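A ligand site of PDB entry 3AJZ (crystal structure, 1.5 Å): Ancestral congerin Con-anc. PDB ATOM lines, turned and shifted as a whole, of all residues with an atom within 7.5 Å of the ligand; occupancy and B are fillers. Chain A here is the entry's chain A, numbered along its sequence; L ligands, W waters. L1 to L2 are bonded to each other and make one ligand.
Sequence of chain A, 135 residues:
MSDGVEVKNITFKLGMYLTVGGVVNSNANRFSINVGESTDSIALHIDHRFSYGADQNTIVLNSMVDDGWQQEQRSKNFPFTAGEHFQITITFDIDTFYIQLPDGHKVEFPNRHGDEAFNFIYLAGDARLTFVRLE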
ATOM      1  N   ARG A  30      -5.153  26.036 -16.202  1.00  0.00           N
ATOM      2  CA  ARG A  30      -4.333  26.657 -17.247  1.00  0.00           C
ATOM      3  C   ARG A  30      -4.514  28.164 -17.186  1.00  0.00           C
ATOM      4  O   ARG A  30      -5.520  28.686 -16.672  1.00  0.00           O
ATOM      5  CB  ARG A  30      -4.759  26.153 -18.625  1.00  0.00           C
ATOM      6  CG  ARG A  30      -6.205  26.573 -18.998  1.00  0.00           C
ATOM      7  CD  ARG A  30      -6.499  26.173 -20.432  1.00  0.00           C
ATOM      8  NE  ARG A  30      -7.880  26.484 -20.810  1.00  0.00           N
ATOM      9  CZ  ARG A  30      -8.263  26.838 -22.035  1.00  0.00           C
ATOM     10  NH1 ARG A  30      -9.544  27.037 -22.281  1.00  0.00           N
ATOM     11  NH2 ARG A  30      -7.380  26.916 -23.039  1.00  0.00           N
ATOM     12  N   SER A  32      -3.469  31.692 -20.021  1.00  0.00           N
ATOM     13  CA  SER A  32      -2.802  32.120 -21.264  1.00  0.00           C
ATOM     14  C   SER A  32      -2.390  33.585 -21.329  1.00  0.00           C
ATOM     15  O   SER A  32      -3.018  34.457 -20.723  1.00  0.00           O
ATOM     16  CB  SER A  32      -3.638  31.765 -22.518  1.00  0.00           C
ATOM     17  OG  SER A  32      -4.897  32.404 -22.430  1.00  0.00           O
ATOM     18  N   ASN A  34      -1.907  36.429 -24.359  1.00  0.00           N
ATOM     19  CA  ASN A  34      -2.502  36.575 -25.704  1.00  0.00           C
ATOM     20  C   ASN A  34      -2.090  37.909 -26.242  1.00  0.00           C
ATOM     21  O   ASN A  34      -2.519  38.916 -25.681  1.00  0.00           O
ATOM     22  CB  ASN A  34      -4.020  36.513 -25.598  1.00  0.00           C
ATOM     23  CG  ASN A  34      -4.488  35.205 -25.041  1.00  0.00           C
ATOM     24  OD1 ASN A  34      -4.683  34.255 -25.799  1.00  0.00           O
ATOM     25  ND2 ASN A  34      -4.681  35.134 -23.729  1.00  0.00           N
ATOM     26  N   HIS A  45      -0.819  33.132 -28.872  1.00  0.00           N
ATOM     27  CA  HIS A  45      -1.512  32.576 -27.716  1.00  0.00           C
ATOM     28  C   HIS A  45      -0.588  31.588 -27.079  1.00  0.00           C
ATOM     29  O   HIS A  45      -0.135  30.638 -27.733  1.00  0.00           O
ATOM     30  CB  HIS A  45      -2.779  31.876 -28.219  1.00  0.00           C
ATOM     31  CG  HIS A  45      -3.476  31.018 -27.194  1.00  0.00           C
ATOM     32  ND1 HIS A  45      -4.232  31.527 -26.156  1.00  0.00           N
ATOM     33  CD2 HIS A  45      -3.629  29.664 -27.142  1.00  0.00           C
ATOM     34  CE1 HIS A  45      -4.806  30.523 -25.498  1.00  0.00           C
ATOM     35  NE2 HIS A  45      -4.442  29.383 -26.065  1.00  0.00           N
ATOM     36  N   ILE A  46      -0.270  31.803 -25.809  1.00  0.00           N
ATOM     37  CA  ILE A  46       0.628  30.900 -25.076  1.00  0.00           C
ATOM     38  C   ILE A  46      -0.194  30.344 -23.939  1.00  0.00           C
ATOM     39  O   ILE A  46      -0.494  31.075 -22.998  1.00  0.00           O
ATOM     40  CB  ILE A  46       1.832  31.683 -24.477  1.00  0.00           C
ATOM     41  CG1 ILE A  46       2.485  32.613 -25.515  1.00  0.00           C
ATOM     42  CG2 ILE A  46       2.835  30.680 -23.915  1.00  0.00           C
ATOM     43  CD1 ILE A  46       3.421  33.643 -24.864  1.00  0.00           C
ATOM     44  N   ASP A  47      -0.592  29.083 -24.051  1.00  0.00           N
ATOM     45  CA  ASP A  47      -1.484  28.469 -23.061  1.00  0.00           C
ATOM     46  C   ASP A  47      -0.661  27.584 -22.157  1.00  0.00           C
ATOM     47  O   ASP A  47      -0.106  26.570 -22.597  1.00  0.00           O
ATOM     48  CB  ASP A  47      -2.586  27.645 -23.760  1.00  0.00           C
ATOM     49  CG  ASP A  47      -3.854  27.527 -22.936  1.00  0.00           C
ATOM     50  OD1 ASP A  47      -4.084  28.383 -22.060  1.00  0.00           O
ATOM     51  OD2 ASP A  47      -4.602  26.560 -23.167  1.00  0.00           O
ATOM     52  N   ARG A  49      -0.665  24.957 -19.720  1.00  0.00           N
ATOM     53  CA  ARG A  49      -1.598  23.935 -19.245  1.00  0.00           C
ATOM     54  C   ARG A  49      -1.027  23.060 -18.149  1.00  0.00           C
ATOM     55  O   ARG A  49      -0.239  22.144 -18.418  1.00  0.00           O
ATOM     56  CB  ARG A  49      -2.082  23.047 -20.413  1.00  0.00           C
ATOM     57  CG  ARG A  49      -2.764  23.891 -21.464  1.00  0.00           C
ATOM     58  CD  ARG A  49      -3.286  23.028 -22.603  1.00  0.00           C
ATOM     59  NE  ARG A  49      -3.991  23.890 -23.534  1.00  0.00           N
ATOM     60  CZ  ARG A  49      -4.641  23.480 -24.616  1.00  0.00           C
ATOM     61  NH1 ARG A  49      -5.255  24.368 -25.382  1.00  0.00           N
ATOM     62  NH2 ARG A  49      -4.654  22.188 -24.953  1.00  0.00           N
ATOM     63  N   TYR A  52      -5.243  20.242 -18.696  1.00  0.00           N
ATOM     64  CA  TYR A  52      -6.355  20.638 -19.523  1.00  0.00           C
ATOM     65  C   TYR A  52      -6.402  19.706 -20.709  1.00  0.00           C
ATOM     66  O   TYR A  52      -5.391  19.485 -21.374  1.00  0.00           O
ATOM     67  CB  TYR A  52      -6.214  22.106 -19.997  1.00  0.00           C
ATOM     68  CG  TYR A  52      -7.318  22.545 -20.953  1.00  0.00           C
ATOM     69  CD1 TYR A  52      -8.527  23.046 -20.471  1.00  0.00           C
ATOM     70  CD2 TYR A  52      -7.131  22.412 -22.320  1.00  0.00           C
ATOM     71  CE1 TYR A  52      -9.549  23.414 -21.356  1.00  0.00           C
ATOM     72  CE2 TYR A  52      -8.131  22.760 -23.206  1.00  0.00           C
ATOM     73  CZ  TYR A  52      -9.323  23.280 -22.711  1.00  0.00           C
ATOM     74  OH  TYR A  52     -10.312  23.602 -23.620  1.00  0.00           O
ATOM     75  N   GLY A  53      -7.574  19.154 -20.997  1.00  0.00           N
ATOM     76  CA  GLY A  53      -7.664  18.234 -22.148  1.00  0.00           C
ATOM     77  C   GLY A  53      -6.732  17.048 -21.946  1.00  0.00           C
ATOM     78  O   GLY A  53      -6.662  16.496 -20.863  1.00  0.00           O
ATOM     79  N   ALA A  54      -5.970  16.700 -22.973  1.00  0.00           N
ATOM     80  CA  ALA A  54      -5.014  15.581 -22.862  1.00  0.00           C
ATOM     81  C   ALA A  54      -3.617  16.034 -22.435  1.00  0.00           C
ATOM     82  O   ALA A  54      -2.654  15.248 -22.433  1.00  0.00           O
ATOM     83  CB  ALA A  54      -4.974  14.762 -24.163  1.00  0.00           C
ATOM     84  N   ASP A  55      -3.518  17.310 -22.049  1.00  0.00           N
ATOM     85  CA  ASP A  55      -2.245  17.933 -21.746  1.00  0.00           C
ATOM     86  C   ASP A  55      -2.019  18.076 -20.249  1.00  0.00           C
ATOM     87  O   ASP A  55      -2.873  18.608 -19.537  1.00  0.00           O
ATOM     88  CB  ASP A  55      -2.159  19.334 -22.372  1.00  0.00           C
ATOM     89  CG  ASP A  55      -2.133  19.283 -23.891  1.00  0.00           C
ATOM     90  OD1 ASP A  55      -1.231  18.624 -24.444  1.00  0.00           O
ATOM     91  OD2 ASP A  55      -3.033  19.868 -24.542  1.00  0.00           O
ATOM     92  N   VAL A  60       0.888  24.962 -24.754  1.00  0.00           N
ATOM     93  CA  VAL A  60       0.305  24.872 -26.089  1.00  0.00           C
ATOM     94  C   VAL A  60       0.298  26.264 -26.678  1.00  0.00           C
ATOM     95  O   VAL A  60      -0.249  27.191 -26.084  1.00  0.00           O
ATOM     96  CB  VAL A  60      -1.118  24.291 -26.013  1.00  0.00           C
ATOM     97  CG1 VAL A  60      -1.767  24.340 -27.396  1.00  0.00           C
ATOM     98  CG2 VAL A  60      -1.036  22.856 -25.458  1.00  0.00           C
ATOM     99  N   LEU A  61       0.935  26.401 -27.829  1.00  0.00           N
ATOM    100  CA  LEU A  61       1.025  27.664 -28.539  1.00  0.00           C
ATOM    101  C   LEU A  61       0.147  27.621 -29.782  1.00  0.00           C
ATOM    102  O   LEU A  61       0.081  26.608 -30.510  1.00  0.00           O
ATOM    103  CB  LEU A  61       2.477  28.014 -28.913  1.00  0.00           C
ATOM    104  CG  LEU A  61       3.387  28.070 -27.684  1.00  0.00           C
ATOM    105  CD1 LEU A  61       4.123  26.733 -27.462  1.00  0.00           C
ATOM    106  CD2 LEU A  61       4.348  29.230 -27.832  1.00  0.00           C
ATOM    107  N   ASN A  62      -0.514  28.717 -30.063  1.00  0.00           N
ATOM    108  CA  ASN A  62      -1.312  28.822 -31.265  1.00  0.00           C
ATOM    109  C   ASN A  62      -1.557  30.297 -31.615  1.00  0.00           C
ATOM    110  O   ASN A  62      -1.077  31.221 -30.951  1.00  0.00           O
ATOM    111  CB  ASN A  62      -2.604  28.022 -31.082  1.00  0.00           C
ATOM    112  CG  ASN A  62      -3.185  27.506 -32.414  1.00  0.00           C
ATOM    113  OD1 ASN A  62      -2.699  27.830 -33.502  1.00  0.00           O
ATOM    114  ND2 ASN A  62      -4.229  26.655 -32.304  1.00  0.00           N
ATOM    115  N   SER A  63      -2.275  30.516 -32.701  1.00  0.00           N
ATOM    116  CA  SER A  63      -2.767  31.795 -33.129  1.00  0.00           C
ATOM    117  C   SER A  63      -4.226  31.647 -33.512  1.00  0.00           C
ATOM    118  O   SER A  63      -4.691  30.521 -33.769  1.00  0.00           O
ATOM    119  CB  SER A  63      -1.965  32.301 -34.336  1.00  0.00           C
ATOM    120  OG  SER A  63      -1.903  31.270 -35.346  1.00  0.00           O
ATOM    121  N   MET A  64      -4.932  32.758 -33.534  1.00  0.00           N
ATOM    122  CA  MET A  64      -6.360  32.788 -33.888  1.00  0.00           C
ATOM    123  C   MET A  64      -6.592  33.849 -34.947  1.00  0.00           C
ATOM    124  O   MET A  64      -6.210  35.009 -34.780  1.00  0.00           O
ATOM    125  CB  MET A  64      -7.192  33.084 -32.629  1.00  0.00           C
ATOM    126  CG  MET A  64      -8.599  33.638 -32.953  1.00  0.00           C
ATOM    127  SD  MET A  64      -9.547  34.023 -31.463  1.00  0.00           S
ATOM    128  CE  MET A  64      -9.785  32.428 -30.858  1.00  0.00           C
ATOM    129  N   TRP A  69      -9.024  29.025 -34.288  1.00  0.00           N
ATOM    130  CA  TRP A  69      -7.678  28.558 -33.949  1.00  0.00           C
ATOM    131  C   TRP A  69      -6.964  27.940 -35.127  1.00  0.00           C
ATOM    132  O   TRP A  69      -7.588  27.286 -35.968  1.00  0.00           O
ATOM    133  CB  TRP A  69      -7.725  27.592 -32.779  1.00  0.00           C
ATOM    134  CG  TRP A  69      -8.178  28.261 -31.505  1.00  0.00           C
ATOM    135  CD1 TRP A  69      -9.368  28.088 -30.881  1.00  0.00           C
ATOM    136  CD2 TRP A  69      -7.447  29.214 -30.732  1.00  0.00           C
ATOM    137  NE1 TRP A  69      -9.436  28.876 -29.756  1.00  0.00           N
ATOM    138  CE2 TRP A  69      -8.267  29.580 -29.642  1.00  0.00           C
ATOM    139  CE3 TRP A  69      -6.182  29.790 -30.857  1.00  0.00           C
ATOM    140  CZ2 TRP A  69      -7.846  30.508 -28.657  1.00  0.00           C
ATOM    141  CZ3 TRP A  69      -5.761  30.707 -29.874  1.00  0.00           C
ATOM    142  CH2 TRP A  69      -6.593  31.047 -28.808  1.00  0.00           C
ATOM    143  N   GLN A  70      -5.649  28.140 -35.187  1.00  0.00           N
ATOM    144  CA  GLN A  70      -4.828  27.575 -36.244  1.00  0.00           C
ATOM    145  C   GLN A  70      -4.119  26.318 -35.728  1.00  0.00           C
ATOM    146  O   GLN A  70      -4.677  25.624 -34.861  1.00  0.00           O
ATOM    147  CB  GLN A  70      -3.876  28.654 -36.803  1.00  0.00           C
ATOM    148  CG  GLN A  70      -4.601  29.897 -37.354  1.00  0.00           C
ATOM    149  CD  GLN A  70      -3.640  30.853 -38.143  1.00  0.00           C
ATOM    150  OE1 GLN A  70      -2.910  31.677 -37.561  1.00  0.00           O
ATOM    151  NE2 GLN A  70      -3.681  30.758 -39.474  1.00  0.00           N
ATOM    152  N   GLN A  71      -2.946  25.975 -36.248  1.00  0.00           N
ATOM    153  CA  GLN A  71      -2.290  24.728 -35.857  1.00  0.00           C
ATOM    154  C   GLN A  71      -1.499  24.879 -34.551  1.00  0.00           C
ATOM    155  O   GLN A  71      -0.633  25.770 -34.394  1.00  0.00           O
ATOM    156  CB  GLN A  71      -1.371  24.207 -36.977  1.00  0.00           C
ATOM    157  CG  GLN A  71      -0.727  22.850 -36.661  1.00  0.00           C
ATOM    158  CD  GLN A  71      -0.212  22.117 -37.910  1.00  0.00           C
ATOM    159  OE1 GLN A  71       0.004  22.715 -38.977  1.00  0.00           O
ATOM    160  NE2 GLN A  71      -0.009  20.809 -37.766  1.00  0.00           N
ATOM    161  N   GLU A  72      -1.764  23.988 -33.616  1.00  0.00           N
ATOM    162  CA  GLU A  72      -1.062  23.969 -32.337  1.00  0.00           C
ATOM    163  C   GLU A  72       0.355  23.528 -32.434  1.00  0.00           C
ATOM    164  O   GLU A  72       0.736  22.683 -33.289  1.00  0.00           O
ATOM    165  CB  GLU A  72      -1.787  23.046 -31.352  1.00  0.00           C
ATOM    166  CG  GLU A  72      -3.128  23.573 -30.980  1.00  0.00           C
ATOM    167  CD  GLU A  72      -3.948  22.633 -30.092  1.00  0.00           C
ATOM    168  OE1 GLU A  72      -3.552  21.468 -29.864  1.00  0.00           O
ATOM    169  OE2 GLU A  72      -5.013  23.067 -29.607  1.00  0.00           O
ATOM    170  N   GLN A  73       1.171  24.133 -31.570  1.00  0.00           N
ATOM    171  CA  GLN A  73       2.510  23.670 -31.317  1.00  0.00           C
ATOM    172  C   GLN A  73       2.634  23.466 -29.828  1.00  0.00           C
ATOM    173  O   GLN A  73       1.903  24.080 -29.039  1.00  0.00           O
ATOM    174  CB  GLN A  73       3.534  24.688 -31.808  1.00  0.00           C
ATOM    175  CG  GLN A  73       3.458  24.891 -33.339  1.00  0.00           C
ATOM    176  CD  GLN A  73       4.592  25.699 -33.947  1.00  0.00           C
ATOM    177  OE1 GLN A  73       5.539  26.196 -33.261  1.00  0.00           O
ATOM    178  NE2 GLN A  73       4.512  25.827 -35.282  1.00  0.00           N
ATOM    179  N   ARG A  74       3.516  22.568 -29.424  1.00  0.00           N
ATOM    180  CA  ARG A  74       3.639  22.225 -28.010  1.00  0.00           C
ATOM    181  C   ARG A  74       5.061  22.318 -27.553  1.00  0.00           C
ATOM    182  O   ARG A  74       5.996  22.063 -28.329  1.00  0.00           O
ATOM    183  CB  ARG A  74       3.083  20.837 -27.710  1.00  0.00           C
ATOM    184  CG  ARG A  74       1.546  20.825 -27.605  1.00  0.00           C
ATOM    185  CD  ARG A  74       0.922  19.423 -27.467  1.00  0.00           C
ATOM    186  NE  ARG A  74      -0.488  19.520 -27.089  1.00  0.00           N
ATOM    187  CZ  ARG A  74      -1.451  19.976 -27.886  1.00  0.00           C
ATOM    188  NH1 ARG A  74      -1.183  20.333 -29.133  1.00  0.00           N
ATOM    189  NH2 ARG A  74      -2.685  20.092 -27.410  1.00  0.00           N
HETATM  190  C1  LIG L   1      -7.263  20.115 -28.294  1.00  0.00           C
HETATM  191  C2  LIG L   1      -7.201  21.338 -27.374  1.00  0.00           C
HETATM  192  C3  LIG L   1      -8.245  22.387 -27.740  1.00  0.00           C
HETATM  193  C4  LIG L   1      -9.592  21.646 -27.732  1.00  0.00           C
HETATM  194  C5  LIG L   1     -10.793  22.524 -28.071  1.00  0.00           C
HETATM  195  C6  LIG L   1      -8.679  19.558 -28.244  1.00  0.00           C
HETATM  196  O1  LIG L   1      -8.813  18.531 -29.194  1.00  0.00           O
HETATM  197  O2  LIG L   1      -6.359  19.131 -27.857  1.00  0.00           O
HETATM  198  O3  LIG L   1      -5.911  21.921 -27.423  1.00  0.00           O
HETATM  199  O4  LIG L   1      -8.284  23.379 -26.736  1.00  0.00           O
HETATM  200  O5  LIG L   1      -9.534  20.594 -28.677  1.00  0.00           O
HETATM  201  O6  LIG L   1     -10.572  23.123 -29.325  1.00  0.00           O
HETATM  202  C1  LG2 L   2      -8.248  24.734 -27.223  1.00  0.00           C
HETATM  203  C2  LG2 L   2      -8.717  25.660 -26.088  1.00  0.00           C
HETATM  204  C3  LG2 L   2      -8.569  27.133 -26.474  1.00  0.00           C
HETATM  205  C4  LG2 L   2      -7.126  27.368 -26.947  1.00  0.00           C
HETATM  206  C5  LG2 L   2      -6.865  26.399 -28.109  1.00  0.00           C
HETATM  207  C6  LG2 L   2      -5.460  26.566 -28.664  1.00  0.00           C
HETATM  208  O1  LG2 L   2     -10.076  25.386 -25.725  1.00  0.00           O
HETATM  209  O2  LG2 L   2      -8.877  27.938 -25.371  1.00  0.00           O
HETATM  210  O3  LG2 L   2      -6.244  27.181 -25.840  1.00  0.00           O
HETATM  211  O4  LG2 L   2      -6.946  25.034 -27.685  1.00  0.00           O
HETATM  212  O5  LG2 L   2      -5.284  25.743 -29.803  1.00  0.00           O
HETATM  213  O   HOH W   1      -4.652  19.105 -30.005  1.00  0.00           O
HETATM  214  O   HOH W   2      -8.009  30.380 -24.149  1.00  0.00           O
HETATM  215  O   HOH W   3      -7.391  24.097 -31.426  1.00  0.00           O
HETATM  216  O   HOH W   4      -5.405  18.550 -25.117  1.00  0.00           O
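Water W1 lies within hydrogen-bond range of OE1 of Glu 72 (2.6 Å), O2 of LIG L1 (2.7 Å) and NH2 of Arg 74 (3.4 Å).
Water W4 lies within hydrogen-bond range of OD2 of Asp 55 (2.8 Å), N of Ala 54 (2.9 Å) and O2 of LIG L1 (3.0 Å).
Water W3 bridges O5 of LG2 L2 (3.1 Å) and OE2 of Glu 72 (3.2 Å).
The side-chain carboxylate (OE2) of Glu 72 is in hydrogen-bond range of an oxygen (O3) of LIG L1, 2.6 Å away.
The side-chain hydroxyl of Tyr 52 lies within hydrogen-bond range of an oxygen (O1) of LG2 L2 (2.8 Å).
NH2 of Arg 49 lies within hydrogen-bond range of O3 of LIG L1 (2.8 Å).
A ring nitrogen (NE2) of His 45 is in hydrogen-bond range of an oxygen (O3) of LG2 L2, at 2.9 Å.
The side-chain amide nitrogen (ND2) of Asn 62 is in hydrogen-bond range of an oxygen (O5) of LG2 L2.
An oxygen (O2) of LG2 L2 is in hydrogen-bond range of the guanidinium group (NH2) of Arg 30, 3.0 Å away.
An oxygen (O3) of LG2 L2 sits at hydrogen-bond distance from the side-chain carboxylate (OD2) of Asp 47, at 3.2 Å.
Residues that only touch the ligand: Trp 69 and Arg 74.
Hydrophobic or aromatic side chains within 4 Å of the ligand: His 45, Tyr 52 and Trp 69.
The nearest printed residue that does not touch the ligand is Val 60 (4.5 Å).
The guanidinium group (NH1) of Arg 74 lies within salt-bridge range of the side-chain carboxylate (OE1) of Glu 72 (2.7 Å).
The guanidinium group (NE) of Arg 49 lies within salt-bridge range of the side-chain carboxylate (OD2) of Asp 47 (2.8 Å).
The guanidinium group of Arg 49 is in salt-bridge range of the side-chain carboxylate of Asp 55, at 2.9 Å.
A ring nitrogen (ND1) of His 45 sits at hydrogen-bond distance from the side-chain amide oxygen (OD1) of Asn 34.
The side-chain amide nitrogen (ND2) of Asn 62 sits at hydrogen-bond distance from the backbone carbonyl oxygen (O) of Gln 70, 2.8 Å away.
The side-chain amide oxygen (OD1) of Asn 62 sits close to the backbone carbonyl oxygen (O) of Gln 71 (3.1 Å).
N of Asp 47 lies within hydrogen-bond range of O of Val 60 (2.8 Å).
The side-chain carboxylate (OD1) of Asp 55 lies within salt-bridge range of the guanidinium group (NE) of Arg 74 (2.9 Å).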
